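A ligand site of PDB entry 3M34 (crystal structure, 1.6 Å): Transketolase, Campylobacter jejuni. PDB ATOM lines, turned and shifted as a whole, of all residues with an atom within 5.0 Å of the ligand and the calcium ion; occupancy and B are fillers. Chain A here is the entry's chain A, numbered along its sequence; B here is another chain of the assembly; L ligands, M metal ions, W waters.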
ATOM      1  N   ALA A  34      22.748  33.556  -8.181  1.00  0.00           N
ATOM      2  CA  ALA A  34      22.015  32.380  -8.648  1.00  0.00           C
ATOM      3  C   ALA A  34      20.671  32.790  -9.258  1.00  0.00           C
ATOM      4  O   ALA A  34      20.333  32.329 -10.328  1.00  0.00           O
ATOM      5  CB  ALA A  34      21.830  31.328  -7.526  1.00  0.00           C
ATOM      6  N   HIS A  70      19.598  29.199  -1.253  1.00  0.00           N
ATOM      7  CA  HIS A  70      20.048  30.568  -1.228  1.00  0.00           C
ATOM      8  C   HIS A  70      19.480  31.375  -2.390  1.00  0.00           C
ATOM      9  O   HIS A  70      19.449  32.601  -2.327  1.00  0.00           O
ATOM     10  CB  HIS A  70      21.580  30.663  -1.165  1.00  0.00           C
ATOM     11  CG  HIS A  70      22.243  30.010  -2.349  1.00  0.00           C
ATOM     12  ND1 HIS A  70      22.391  28.644  -2.448  1.00  0.00           N
ATOM     13  CD2 HIS A  70      22.793  30.537  -3.473  1.00  0.00           C
ATOM     14  CE1 HIS A  70      22.976  28.362  -3.606  1.00  0.00           C
ATOM     15  NE2 HIS A  70      23.222  29.501  -4.245  1.00  0.00           N
ATOM     16  N   GLY A 117      18.379  24.820   1.829  1.00  0.00           N
ATOM     17  CA  GLY A 117      19.360  25.702   2.473  1.00  0.00           C
ATOM     18  C   GLY A 117      20.648  24.945   2.721  1.00  0.00           C
ATOM     19  O   GLY A 117      21.680  25.254   2.073  1.00  0.00           O
ATOM     20  N   PRO A 118      20.566  23.905   3.544  1.00  0.00           N
ATOM     21  CA  PRO A 118      21.730  23.014   3.676  1.00  0.00           C
ATOM     22  C   PRO A 118      21.941  22.295   2.380  1.00  0.00           C
ATOM     23  O   PRO A 118      21.038  21.588   1.874  1.00  0.00           O
ATOM     24  CB  PRO A 118      21.354  22.068   4.797  1.00  0.00           C
ATOM     25  CG  PRO A 118      20.122  22.752   5.483  1.00  0.00           C
ATOM     26  CD  PRO A 118      19.451  23.486   4.383  1.00  0.00           C
ATOM     27  N   LEU A 119      23.087  22.468   1.780  1.00  0.00           N
ATOM     28  CA  LEU A 119      23.306  22.008   0.397  1.00  0.00           C
ATOM     29  C   LEU A 119      23.282  20.483   0.295  1.00  0.00           C
ATOM     30  O   LEU A 119      23.599  19.775   1.267  1.00  0.00           O
ATOM     31  CB  LEU A 119      24.642  22.559  -0.129  1.00  0.00           C
ATOM     32  CG  LEU A 119      24.629  24.057  -0.491  1.00  0.00           C
ATOM     33  CD1 LEU A 119      26.095  24.547  -0.649  1.00  0.00           C
ATOM     34  CD2 LEU A 119      23.790  24.391  -1.729  1.00  0.00           C
ATOM     35  N   GLY A 154      23.021  23.425  -7.736  1.00  0.00           N
ATOM     36  CA  GLY A 154      24.254  24.104  -8.105  1.00  0.00           C
ATOM     37  C   GLY A 154      25.462  23.273  -7.801  1.00  0.00           C
ATOM     38  O   GLY A 154      25.350  22.118  -7.385  1.00  0.00           O
ATOM     39  N   ASP A 155      26.617  23.881  -7.935  1.00  0.00           N
ATOM     40  CA  ASP A 155      27.874  23.167  -7.672  1.00  0.00           C
ATOM     41  C   ASP A 155      27.939  22.630  -6.268  1.00  0.00           C
ATOM     42  O   ASP A 155      28.468  21.535  -6.006  1.00  0.00           O
ATOM     43  CB  ASP A 155      29.024  24.113  -7.874  1.00  0.00           C
ATOM     44  CG  ASP A 155      29.122  24.599  -9.317  1.00  0.00           C
ATOM     45  OD1 ASP A 155      29.415  23.791 -10.217  1.00  0.00           O
ATOM     46  OD2 ASP A 155      28.961  25.826  -9.574  1.00  0.00           O
ATOM     47  N   GLY A 156      27.461  23.418  -5.336  1.00  0.00           N
ATOM     48  CA  GLY A 156      27.577  23.033  -3.962  1.00  0.00           C
ATOM     49  C   GLY A 156      26.792  21.760  -3.667  1.00  0.00           C
ATOM     50  O   GLY A 156      27.221  20.891  -2.894  1.00  0.00           O
ATOM     51  N   ASP A 157      25.578  21.680  -4.218  1.00  0.00           N
ATOM     52  CA  ASP A 157      24.764  20.495  -4.057  1.00  0.00           C
ATOM     53  C   ASP A 157      25.502  19.239  -4.543  1.00  0.00           C
ATOM     54  O   ASP A 157      25.461  18.206  -3.903  1.00  0.00           O
ATOM     55  CB  ASP A 157      23.438  20.643  -4.806  1.00  0.00           C
ATOM     56  CG  ASP A 157      22.610  21.740  -4.254  1.00  0.00           C
ATOM     57  OD1 ASP A 157      22.098  21.590  -3.094  1.00  0.00           O
ATOM     58  OD2 ASP A 157      22.393  22.743  -4.968  1.00  0.00           O
ATOM     59  N   GLU A 160      28.356  17.725  -2.437  1.00  0.00           N
ATOM     60  CA  GLU A 160      27.988  17.011  -1.197  1.00  0.00           C
ATOM     61  C   GLU A 160      27.735  15.522  -1.436  1.00  0.00           C
ATOM     62  O   GLU A 160      27.088  15.131  -2.417  1.00  0.00           O
ATOM     63  CB  GLU A 160      26.744  17.653  -0.607  1.00  0.00           C
ATOM     64  CG  GLU A 160      26.956  19.010  -0.016  1.00  0.00           C
ATOM     65  CD  GLU A 160      27.668  18.952   1.358  1.00  0.00           C
ATOM     66  OE1 GLU A 160      27.991  17.850   1.813  1.00  0.00           O
ATOM     67  OE2 GLU A 160      27.917  20.012   1.950  1.00  0.00           O
ATOM     68  N   ASP A 183      22.775  23.950 -12.432  1.00  0.00           N
ATOM     69  CA  ASP A 183      23.292  25.276 -12.751  1.00  0.00           C
ATOM     70  C   ASP A 183      24.825  25.277 -12.695  1.00  0.00           C
ATOM     71  O   ASP A 183      25.431  25.426 -11.638  1.00  0.00           O
ATOM     72  CB  ASP A 183      22.722  26.339 -11.793  1.00  0.00           C
ATOM     73  CG  ASP A 183      23.137  27.738 -12.151  1.00  0.00           C
ATOM     74  OD1 ASP A 183      23.782  27.862 -13.225  1.00  0.00           O
ATOM     75  OD2 ASP A 183      22.851  28.698 -11.363  1.00  0.00           O
ATOM     76  N   ASN A 185      27.841  27.147 -13.291  1.00  0.00           N
ATOM     77  CA  ASN A 185      28.330  28.502 -13.518  1.00  0.00           C
ATOM     78  C   ASN A 185      29.818  28.726 -13.224  1.00  0.00           C
ATOM     79  O   ASN A 185      30.300  29.844 -13.295  1.00  0.00           O
ATOM     80  CB  ASN A 185      27.409  29.521 -12.837  1.00  0.00           C
ATOM     81  CG  ASN A 185      27.398  29.398 -11.346  1.00  0.00           C
ATOM     82  OD1 ASN A 185      28.317  28.799 -10.727  1.00  0.00           O
ATOM     83  ND2 ASN A 185      26.367  30.010 -10.707  1.00  0.00           N
ATOM     84  N   ASN A 186      30.506  27.638 -12.869  1.00  0.00           N
ATOM     85  CA  ASN A 186      31.936  27.634 -12.611  1.00  0.00           C
ATOM     86  C   ASN A 186      32.379  28.493 -11.424  1.00  0.00           C
ATOM     87  O   ASN A 186      33.569  28.742 -11.289  1.00  0.00           O
ATOM     88  CB  ASN A 186      32.754  28.042 -13.842  1.00  0.00           C
ATOM     89  CG  ASN A 186      34.227  27.672 -13.711  1.00  0.00           C
ATOM     90  OD1 ASN A 186      35.130  28.526 -13.906  1.00  0.00           O
ATOM     91  ND2 ASN A 186      34.488  26.420 -13.334  1.00  0.00           N
ATOM     92  N   ILE A 187      31.440  28.936 -10.576  1.00  0.00           N
ATOM     93  CA  ILE A 187      31.756  29.819  -9.462  1.00  0.00           C
ATOM     94  C   ILE A 187      31.188  29.307  -8.156  1.00  0.00           C
ATOM     95  O   ILE A 187      30.058  28.796  -8.127  1.00  0.00           O
ATOM     96  CB  ILE A 187      31.168  31.244  -9.748  1.00  0.00           C
ATOM     97  CG1 ILE A 187      31.969  31.890 -10.918  1.00  0.00           C
ATOM     98  CG2 ILE A 187      31.059  32.080  -8.442  1.00  0.00           C
ATOM     99  CD1 ILE A 187      33.363  32.304 -10.544  1.00  0.00           C
ATOM    100  N   SER A 188      32.004  29.385  -7.103  1.00  0.00           N
ATOM    101  CA  SER A 188      31.514  29.141  -5.725  1.00  0.00           C
ATOM    102  C   SER A 188      32.053  30.237  -4.823  1.00  0.00           C
ATOM    103  O   SER A 188      32.600  31.222  -5.300  1.00  0.00           O
ATOM    104  CB  SER A 188      31.842  27.693  -5.252  1.00  0.00           C
ATOM    105  OG  SER A 188      33.205  27.584  -5.022  1.00  0.00           O
ATOM    106  N   ILE A 189      31.877  30.123  -3.493  1.00  0.00           N
ATOM    107  CA  ILE A 189      32.300  31.222  -2.624  1.00  0.00           C
ATOM    108  C   ILE A 189      33.815  31.457  -2.685  1.00  0.00           C
ATOM    109  O   ILE A 189      34.268  32.590  -2.609  1.00  0.00           O
ATOM    110  CB  ILE A 189      31.810  30.975  -1.183  1.00  0.00           C
ATOM    111  CG1 ILE A 189      30.279  31.139  -1.134  1.00  0.00           C
ATOM    112  CG2 ILE A 189      32.473  31.898  -0.212  1.00  0.00           C
ATOM    113  CD1 ILE A 189      29.700  30.766   0.207  1.00  0.00           C
ATOM    114  N   VAL A 193      35.360  27.126  -9.479  1.00  0.00           N
ATOM    115  CA  VAL A 193      34.987  25.783  -8.980  1.00  0.00           C
ATOM    116  C   VAL A 193      36.121  24.815  -9.233  1.00  0.00           C
ATOM    117  O   VAL A 193      36.307  23.878  -8.500  1.00  0.00           O
ATOM    118  CB  VAL A 193      33.692  25.310  -9.677  1.00  0.00           C
ATOM    119  CG1 VAL A 193      33.576  23.758  -9.683  1.00  0.00           C
ATOM    120  CG2 VAL A 193      32.517  25.937  -8.933  1.00  0.00           C
ATOM    121  N   ILE A 245      26.980  33.296 -13.621  1.00  0.00           N
ATOM    122  CA  ILE A 245      26.449  33.825 -12.390  1.00  0.00           C
ATOM    123  C   ILE A 245      26.199  35.345 -12.562  1.00  0.00           C
ATOM    124  O   ILE A 245      26.973  36.045 -13.172  1.00  0.00           O
ATOM    125  CB  ILE A 245      27.334  33.451 -11.174  1.00  0.00           C
ATOM    126  CG1 ILE A 245      26.555  33.680  -9.861  1.00  0.00           C
ATOM    127  CG2 ILE A 245      28.609  34.290 -11.103  1.00  0.00           C
ATOM    128  CD1 ILE A 245      27.306  33.201  -8.612  1.00  0.00           C
ATOM    129  N   HIS A 259      27.734  36.181  -5.457  1.00  0.00           N
ATOM    130  CA  HIS A 259      27.086  34.998  -4.906  1.00  0.00           C
ATOM    131  C   HIS A 259      26.158  35.375  -3.765  1.00  0.00           C
ATOM    132  O   HIS A 259      25.019  34.898  -3.694  1.00  0.00           O
ATOM    133  CB  HIS A 259      28.121  33.968  -4.415  1.00  0.00           C
ATOM    134  CG  HIS A 259      27.562  32.972  -3.454  1.00  0.00           C
ATOM    135  ND1 HIS A 259      26.843  31.867  -3.853  1.00  0.00           N
ATOM    136  CD2 HIS A 259      27.526  32.969  -2.094  1.00  0.00           C
ATOM    137  CE1 HIS A 259      26.403  31.225  -2.783  1.00  0.00           C
ATOM    138  NE2 HIS A 259      26.772  31.889  -1.706  1.00  0.00           N
ATOM    139  N   ALA B 366      35.465  24.321   3.860  1.00  0.00           N
ATOM    140  CA  ALA B 366      34.613  23.701   2.900  1.00  0.00           C
ATOM    141  C   ALA B 366      33.883  24.754   2.083  1.00  0.00           C
ATOM    142  O   ALA B 366      32.711  25.006   2.274  1.00  0.00           O
ATOM    143  CB  ALA B 366      33.621  22.729   3.581  1.00  0.00           C
ATOM    144  N   ASP B 367      34.632  25.362   1.155  1.00  0.00           N
ATOM    145  CA  ASP B 367      34.184  26.458   0.288  1.00  0.00           C
ATOM    146  C   ASP B 367      33.869  27.758   1.013  1.00  0.00           C
ATOM    147  O   ASP B 367      33.277  28.616   0.401  1.00  0.00           O
ATOM    148  CB  ASP B 367      33.027  26.071  -0.624  1.00  0.00           C
ATOM    149  CG  ASP B 367      32.810  27.064  -1.788  1.00  0.00           C
ATOM    150  OD1 ASP B 367      33.820  27.451  -2.460  1.00  0.00           O
ATOM    151  OD2 ASP B 367      31.673  27.510  -2.009  1.00  0.00           O
ATOM    152  N   LEU B 368      34.201  27.912   2.310  1.00  0.00           N
ATOM    153  CA  LEU B 368      33.815  29.112   3.026  1.00  0.00           C
ATOM    154  C   LEU B 368      34.990  29.931   3.588  1.00  0.00           C
ATOM    155  O   LEU B 368      34.820  30.765   4.505  1.00  0.00           O
ATOM    156  CB  LEU B 368      32.862  28.778   4.179  1.00  0.00           C
ATOM    157  CG  LEU B 368      31.501  28.311   3.732  1.00  0.00           C
ATOM    158  CD1 LEU B 368      30.778  27.648   4.921  1.00  0.00           C
ATOM    159  CD2 LEU B 368      30.699  29.499   3.235  1.00  0.00           C
ATOM    160  N   ILE B 392      32.672  21.810  -1.265  1.00  0.00           N
ATOM    161  CA  ILE B 392      31.527  21.678  -0.391  1.00  0.00           C
ATOM    162  C   ILE B 392      31.410  20.200   0.077  1.00  0.00           C
ATOM    163  O   ILE B 392      30.502  19.452  -0.335  1.00  0.00           O
ATOM    164  CB  ILE B 392      30.223  22.233  -1.041  1.00  0.00           C
ATOM    165  CG1 ILE B 392      30.364  23.701  -1.491  1.00  0.00           C
ATOM    166  CG2 ILE B 392      29.076  22.179   0.033  1.00  0.00           C
ATOM    167  CD1 ILE B 392      31.117  23.907  -2.839  1.00  0.00           C
ATOM    168  N   GLU B 394      32.122  18.820   3.667  1.00  0.00           N
ATOM    169  CA  GLU B 394      32.498  18.987   5.064  1.00  0.00           C
ATOM    170  C   GLU B 394      32.969  17.637   5.644  1.00  0.00           C
ATOM    171  O   GLU B 394      33.952  17.601   6.402  1.00  0.00           O
ATOM    172  CB  GLU B 394      31.333  19.499   5.923  1.00  0.00           C
ATOM    173  CG  GLU B 394      30.819  20.844   5.609  1.00  0.00           C
ATOM    174  CD  GLU B 394      29.867  20.918   4.459  1.00  0.00           C
ATOM    175  OE1 GLU B 394      29.429  19.838   3.951  1.00  0.00           O
ATOM    176  OE2 GLU B 394      29.525  22.061   4.126  1.00  0.00           O
ATOM    177  N   THR B 416      34.159  25.294   8.800  1.00  0.00           N
ATOM    178  CA  THR B 416      32.894  25.517   8.159  1.00  0.00           C
ATOM    179  C   THR B 416      32.030  26.405   9.106  1.00  0.00           C
ATOM    180  O   THR B 416      32.452  26.742  10.194  1.00  0.00           O
ATOM    181  CB  THR B 416      32.131  24.205   7.754  1.00  0.00           C
ATOM    182  OG1 THR B 416      30.913  24.501   7.009  1.00  0.00           O
ATOM    183  CG2 THR B 416      31.915  23.240   8.962  1.00  0.00           C
ATOM    184  N   PHE B 417      30.796  26.667   8.682  1.00  0.00           N
ATOM    185  CA  PHE B 417      29.795  27.273   9.612  1.00  0.00           C
ATOM    186  C   PHE B 417      29.422  26.245  10.670  1.00  0.00           C
ATOM    187  O   PHE B 417      29.312  25.025  10.441  1.00  0.00           O
ATOM    188  CB  PHE B 417      28.478  27.691   8.932  1.00  0.00           C
ATOM    189  CG  PHE B 417      28.598  28.803   7.887  1.00  0.00           C
ATOM    190  CD1 PHE B 417      29.555  29.823   7.996  1.00  0.00           C
ATOM    191  CD2 PHE B 417      27.717  28.824   6.795  1.00  0.00           C
ATOM    192  CE1 PHE B 417      29.630  30.835   7.042  1.00  0.00           C
ATOM    193  CE2 PHE B 417      27.787  29.836   5.819  1.00  0.00           C
ATOM    194  CZ  PHE B 417      28.754  30.858   5.972  1.00  0.00           C
ATOM    195  N   PHE B 420      26.864  23.611   9.966  1.00  0.00           N
ATOM    196  CA  PHE B 420      27.300  22.503   9.130  1.00  0.00           C
ATOM    197  C   PHE B 420      28.358  21.648   9.716  1.00  0.00           C
ATOM    198  O   PHE B 420      28.801  20.627   9.101  1.00  0.00           O
ATOM    199  CB  PHE B 420      27.563  22.958   7.706  1.00  0.00           C
ATOM    200  CG  PHE B 420      26.393  23.723   7.111  1.00  0.00           C
ATOM    201  CD1 PHE B 420      25.116  23.216   7.237  1.00  0.00           C
ATOM    202  CD2 PHE B 420      26.546  24.945   6.528  1.00  0.00           C
ATOM    203  CE1 PHE B 420      24.033  23.890   6.735  1.00  0.00           C
ATOM    204  CE2 PHE B 420      25.478  25.621   6.018  1.00  0.00           C
ATOM    205  CZ  PHE B 420      24.202  25.081   6.163  1.00  0.00           C
ATOM    206  N   TYR B 423      27.373  17.993   9.406  1.00  0.00           N
ATOM    207  CA  TYR B 423      27.754  17.220   8.220  1.00  0.00           C
ATOM    208  C   TYR B 423      29.042  16.463   8.467  1.00  0.00           C
ATOM    209  O   TYR B 423      29.253  15.430   7.831  1.00  0.00           O
ATOM    210  CB  TYR B 423      27.898  18.079   6.962  1.00  0.00           C
ATOM    211  CG  TYR B 423      26.632  18.411   6.208  1.00  0.00           C
ATOM    212  CD1 TYR B 423      25.634  19.200   6.766  1.00  0.00           C
ATOM    213  CD2 TYR B 423      26.492  18.053   4.865  1.00  0.00           C
ATOM    214  CE1 TYR B 423      24.522  19.525   6.065  1.00  0.00           C
ATOM    215  CE2 TYR B 423      25.352  18.369   4.162  1.00  0.00           C
ATOM    216  CZ  TYR B 423      24.393  19.127   4.735  1.00  0.00           C
ATOM    217  OH  TYR B 423      23.264  19.469   4.005  1.00  0.00           O
ATOM    218  N   HIS B 456      20.286  28.039   9.120  1.00  0.00           N
ATOM    219  CA  HIS B 456      21.685  28.489   9.212  1.00  0.00           C
ATOM    220  C   HIS B 456      22.032  28.973  10.615  1.00  0.00           C
ATOM    221  O   HIS B 456      23.097  29.565  10.804  1.00  0.00           O
ATOM    222  CB  HIS B 456      21.941  29.564   8.193  1.00  0.00           C
ATOM    223  CG  HIS B 456      22.061  29.019   6.802  1.00  0.00           C
ATOM    224  ND1 HIS B 456      23.189  29.197   6.018  1.00  0.00           N
ATOM    225  CD2 HIS B 456      21.171  28.359   6.044  1.00  0.00           C
ATOM    226  CE1 HIS B 456      22.989  28.589   4.865  1.00  0.00           C
ATOM    227  NE2 HIS B 456      21.775  28.073   4.858  1.00  0.00           N
HETATM  228  N1  LIG L   1      27.532  23.739   3.427  1.00  0.00           N
HETATM  229  C1  LIG L   1      26.258  23.246   3.350  1.00  0.00           C
HETATM  230  C2  LIG L   1      25.974  21.787   3.717  1.00  0.00           C
HETATM  231  N2  LIG L   1      25.239  24.089   3.058  1.00  0.00           N
HETATM  232  C3  LIG L   1      25.475  25.384   2.798  1.00  0.00           C
HETATM  233  N3  LIG L   1      24.453  26.208   2.521  1.00  0.00           N
HETATM  234  C4  LIG L   1      26.797  25.910   2.813  1.00  0.00           C
HETATM  235  C5  LIG L   1      27.796  25.018   3.166  1.00  0.00           C
HETATM  236  C6  LIG L   1      27.133  27.373   2.507  1.00  0.00           C
HETATM  237  N4  LIG L   1      26.977  27.653   1.058  1.00  0.00           N
HETATM  238  C7  LIG L   1      25.870  28.245   0.541  1.00  0.00           C
HETATM  239  S1  LIG L   1      25.975  28.293  -1.176  1.00  0.00           S
HETATM  240  C8  LIG L   1      27.617  27.766  -1.161  1.00  0.00           C
HETATM  241  C9  LIG L   1      27.927  27.389   0.133  1.00  0.00           C
HETATM  242  C10 LIG L   1      29.284  26.832   0.511  1.00  0.00           C
HETATM  243  C11 LIG L   1      28.357  27.653  -2.460  1.00  0.00           C
HETATM  244  C12 LIG L   1      27.354  26.990  -3.344  1.00  0.00           C
HETATM  245  O1  LIG L   1      27.637  27.338  -4.568  1.00  0.00           O
HETATM  246  P1  LIG L   1      26.695  27.083  -5.652  1.00  0.00           P
HETATM  247  O2  LIG L   1      27.912  26.835  -6.476  1.00  0.00           O
HETATM  248  O3  LIG L   1      26.045  25.902  -5.092  1.00  0.00           O
HETATM  249  O4  LIG L   1      26.157  28.425  -5.465  1.00  0.00           O
HETATM  250  P2  LIG L   1      25.984  29.570  -6.597  1.00  0.00           P
HETATM  251  O5  LIG L   1      27.181  30.335  -6.080  1.00  0.00           O
HETATM  252  O6  LIG L   1      26.632  29.287  -7.985  1.00  0.00           O
HETATM  253  O7  LIG L   1      24.978  30.543  -6.373  1.00  0.00           O
HETATM  254 CA    CA M   1      28.078  27.749  -8.649  1.00  0.00          CA
HETATM  255  O   HOH W   1      26.016  26.789  -9.356  1.00  0.00           O
HETATM  256  O   HOH W   2      23.684  27.997  -8.705  1.00  0.00           O
HETATM  257  O   HOH W   3      23.316  25.566  -5.041  1.00  0.00           O
HETATM  258  O   HOH W   4      30.818  24.439   4.377  1.00  0.00           O
HETATM  259  O   HOH W   5      24.064  33.057  -5.618  1.00  0.00           O
HETATM  260  O   HOH W   6      22.882  29.064   1.849  1.00  0.00           O
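Water W1 bridges the backbone carbonyl oxygen of Asp 183 (2.7 Å) and the backbone NH of Asp 155 (3.3 Å). Water W3 lies within hydrogen-bond range of O3 of the ligand (2.8 Å), OD2 of Asp 157 (3.0 Å) and N of Gly 154 (3.5 Å). Water W5 lies within hydrogen-bond range of O7 of the ligand (2.8 Å), O of His 259 (2.8 Å) and N of Ala 34 (2.9 Å). Water W6 lies within hydrogen-bond range of N3 of the ligand and NE2 of His 456 of chain B.
The side-chain carboxylate (OE1) of Glu 394 of chain B sits close to the side-chain carboxylate (OE2) of Glu 160, 2.5 Å away. The side-chain hydroxyl (OH) of Tyr 423 of chain B lies within hydrogen-bond range of the backbone carbonyl oxygen (O) of Leu 119, 2.8 Å away. The backbone NH (N) of Glu 160 lies close to the backbone carbonyl oxygen (O) of Ile 392 of chain B, at 3.5 Å. The side-chain carboxylate of Asp 367 of chain B sits at hydrogen-bond distance from the backbone NH of Ile 189 (3.0 Å). The side-chain carboxylate (OD1) of Asp 367 of chain B sits at hydrogen-bond distance from the side-chain hydroxyl (OG) of Ser 188 (2.6 Å). The backbone NH of Gly 154 lies within hydrogen-bond range of the side-chain carboxylate of Asp 157 (2.9 Å).
OE2 of Glu 394 of chain B lies within hydrogen-bond range of N1 of the ligand (2.7 Å). A ring nitrogen (ND1) of His 259 lies within hydrogen-bond range of an oxygen (O5) of the ligand (2.7 Å). An oxygen (O3) of the ligand lies within hydrogen-bond range of the backbone NH of Gly 156. An oxygen (O7) of the ligand is in hydrogen-bond range of a ring nitrogen (NE2) of His 70, at 2.9 Å. O of Gly 117 lies within hydrogen-bond range of N3 of the ligand (3.0 Å). N of Leu 119 is in hydrogen-bond range of N2 of the ligand (3.0 Å).
Ala 34 touches the ligand. CA of Pro 118 touches N2 of the ligand, at 3.7 Å. C of Gly 154 touches O3 of the ligand, 3.8 Å away. OE2 of Glu 160 touches C2 of the ligand (3.2 Å). CD1 of Ile 189 touches C9 of the ligand (3.8 Å). CD1 of Ile 245 touches O5 of the ligand (3.8 Å). Asp 367 of chain B touches the ligand (OD2 to C11, 3.3 Å). CG1 of Ile 392 of chain B touches C10 of the ligand (3.9 Å). Phe 420 of chain B touches the ligand (CE2 to C3, 3.2 Å). CZ of Tyr 423 of chain B touches C2 of the ligand (3.3 Å). His 456 of chain B touches the ligand (CE1 to N3, 3.6 Å). Hydrophobic or aromatic side chains that line the ligand: Ala 34, His 70, Leu 119, Ile 189, Ile 245, His 259, Ile 392 of chain B, Phe 420 of chain B, Tyr 423 of chain B and His 456 of chain B. Within 4 Å of the ligand: Ala 34, His 70, Gly 117, Pro 118, Leu 119, Gly 154, Asp 155, Gly 156, Glu 160, Asn 185, Ile 187, Ile 189, Ile 245, His 259, Asp 367 of chain B, Ile 392 of chain B, Glu 394 of chain B, Phe 420 of chain B, Tyr 423 of chain B and His 456 of chain B.
Within 4 Å of the calcium ion: Asp 155, Asn 185 and Ile 187.
The calcium ion is bound by O6 of the ligand (2.2 Å), O of Ile 187 (2.3 Å), OD2 of Asp 155 (2.3 Å), OD1 of Asn 185 (2.3 Å), O2 of the ligand (2.4 Å) and water W1 (2.4 Å). The calcium ion has six donor atoms within binding distance.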
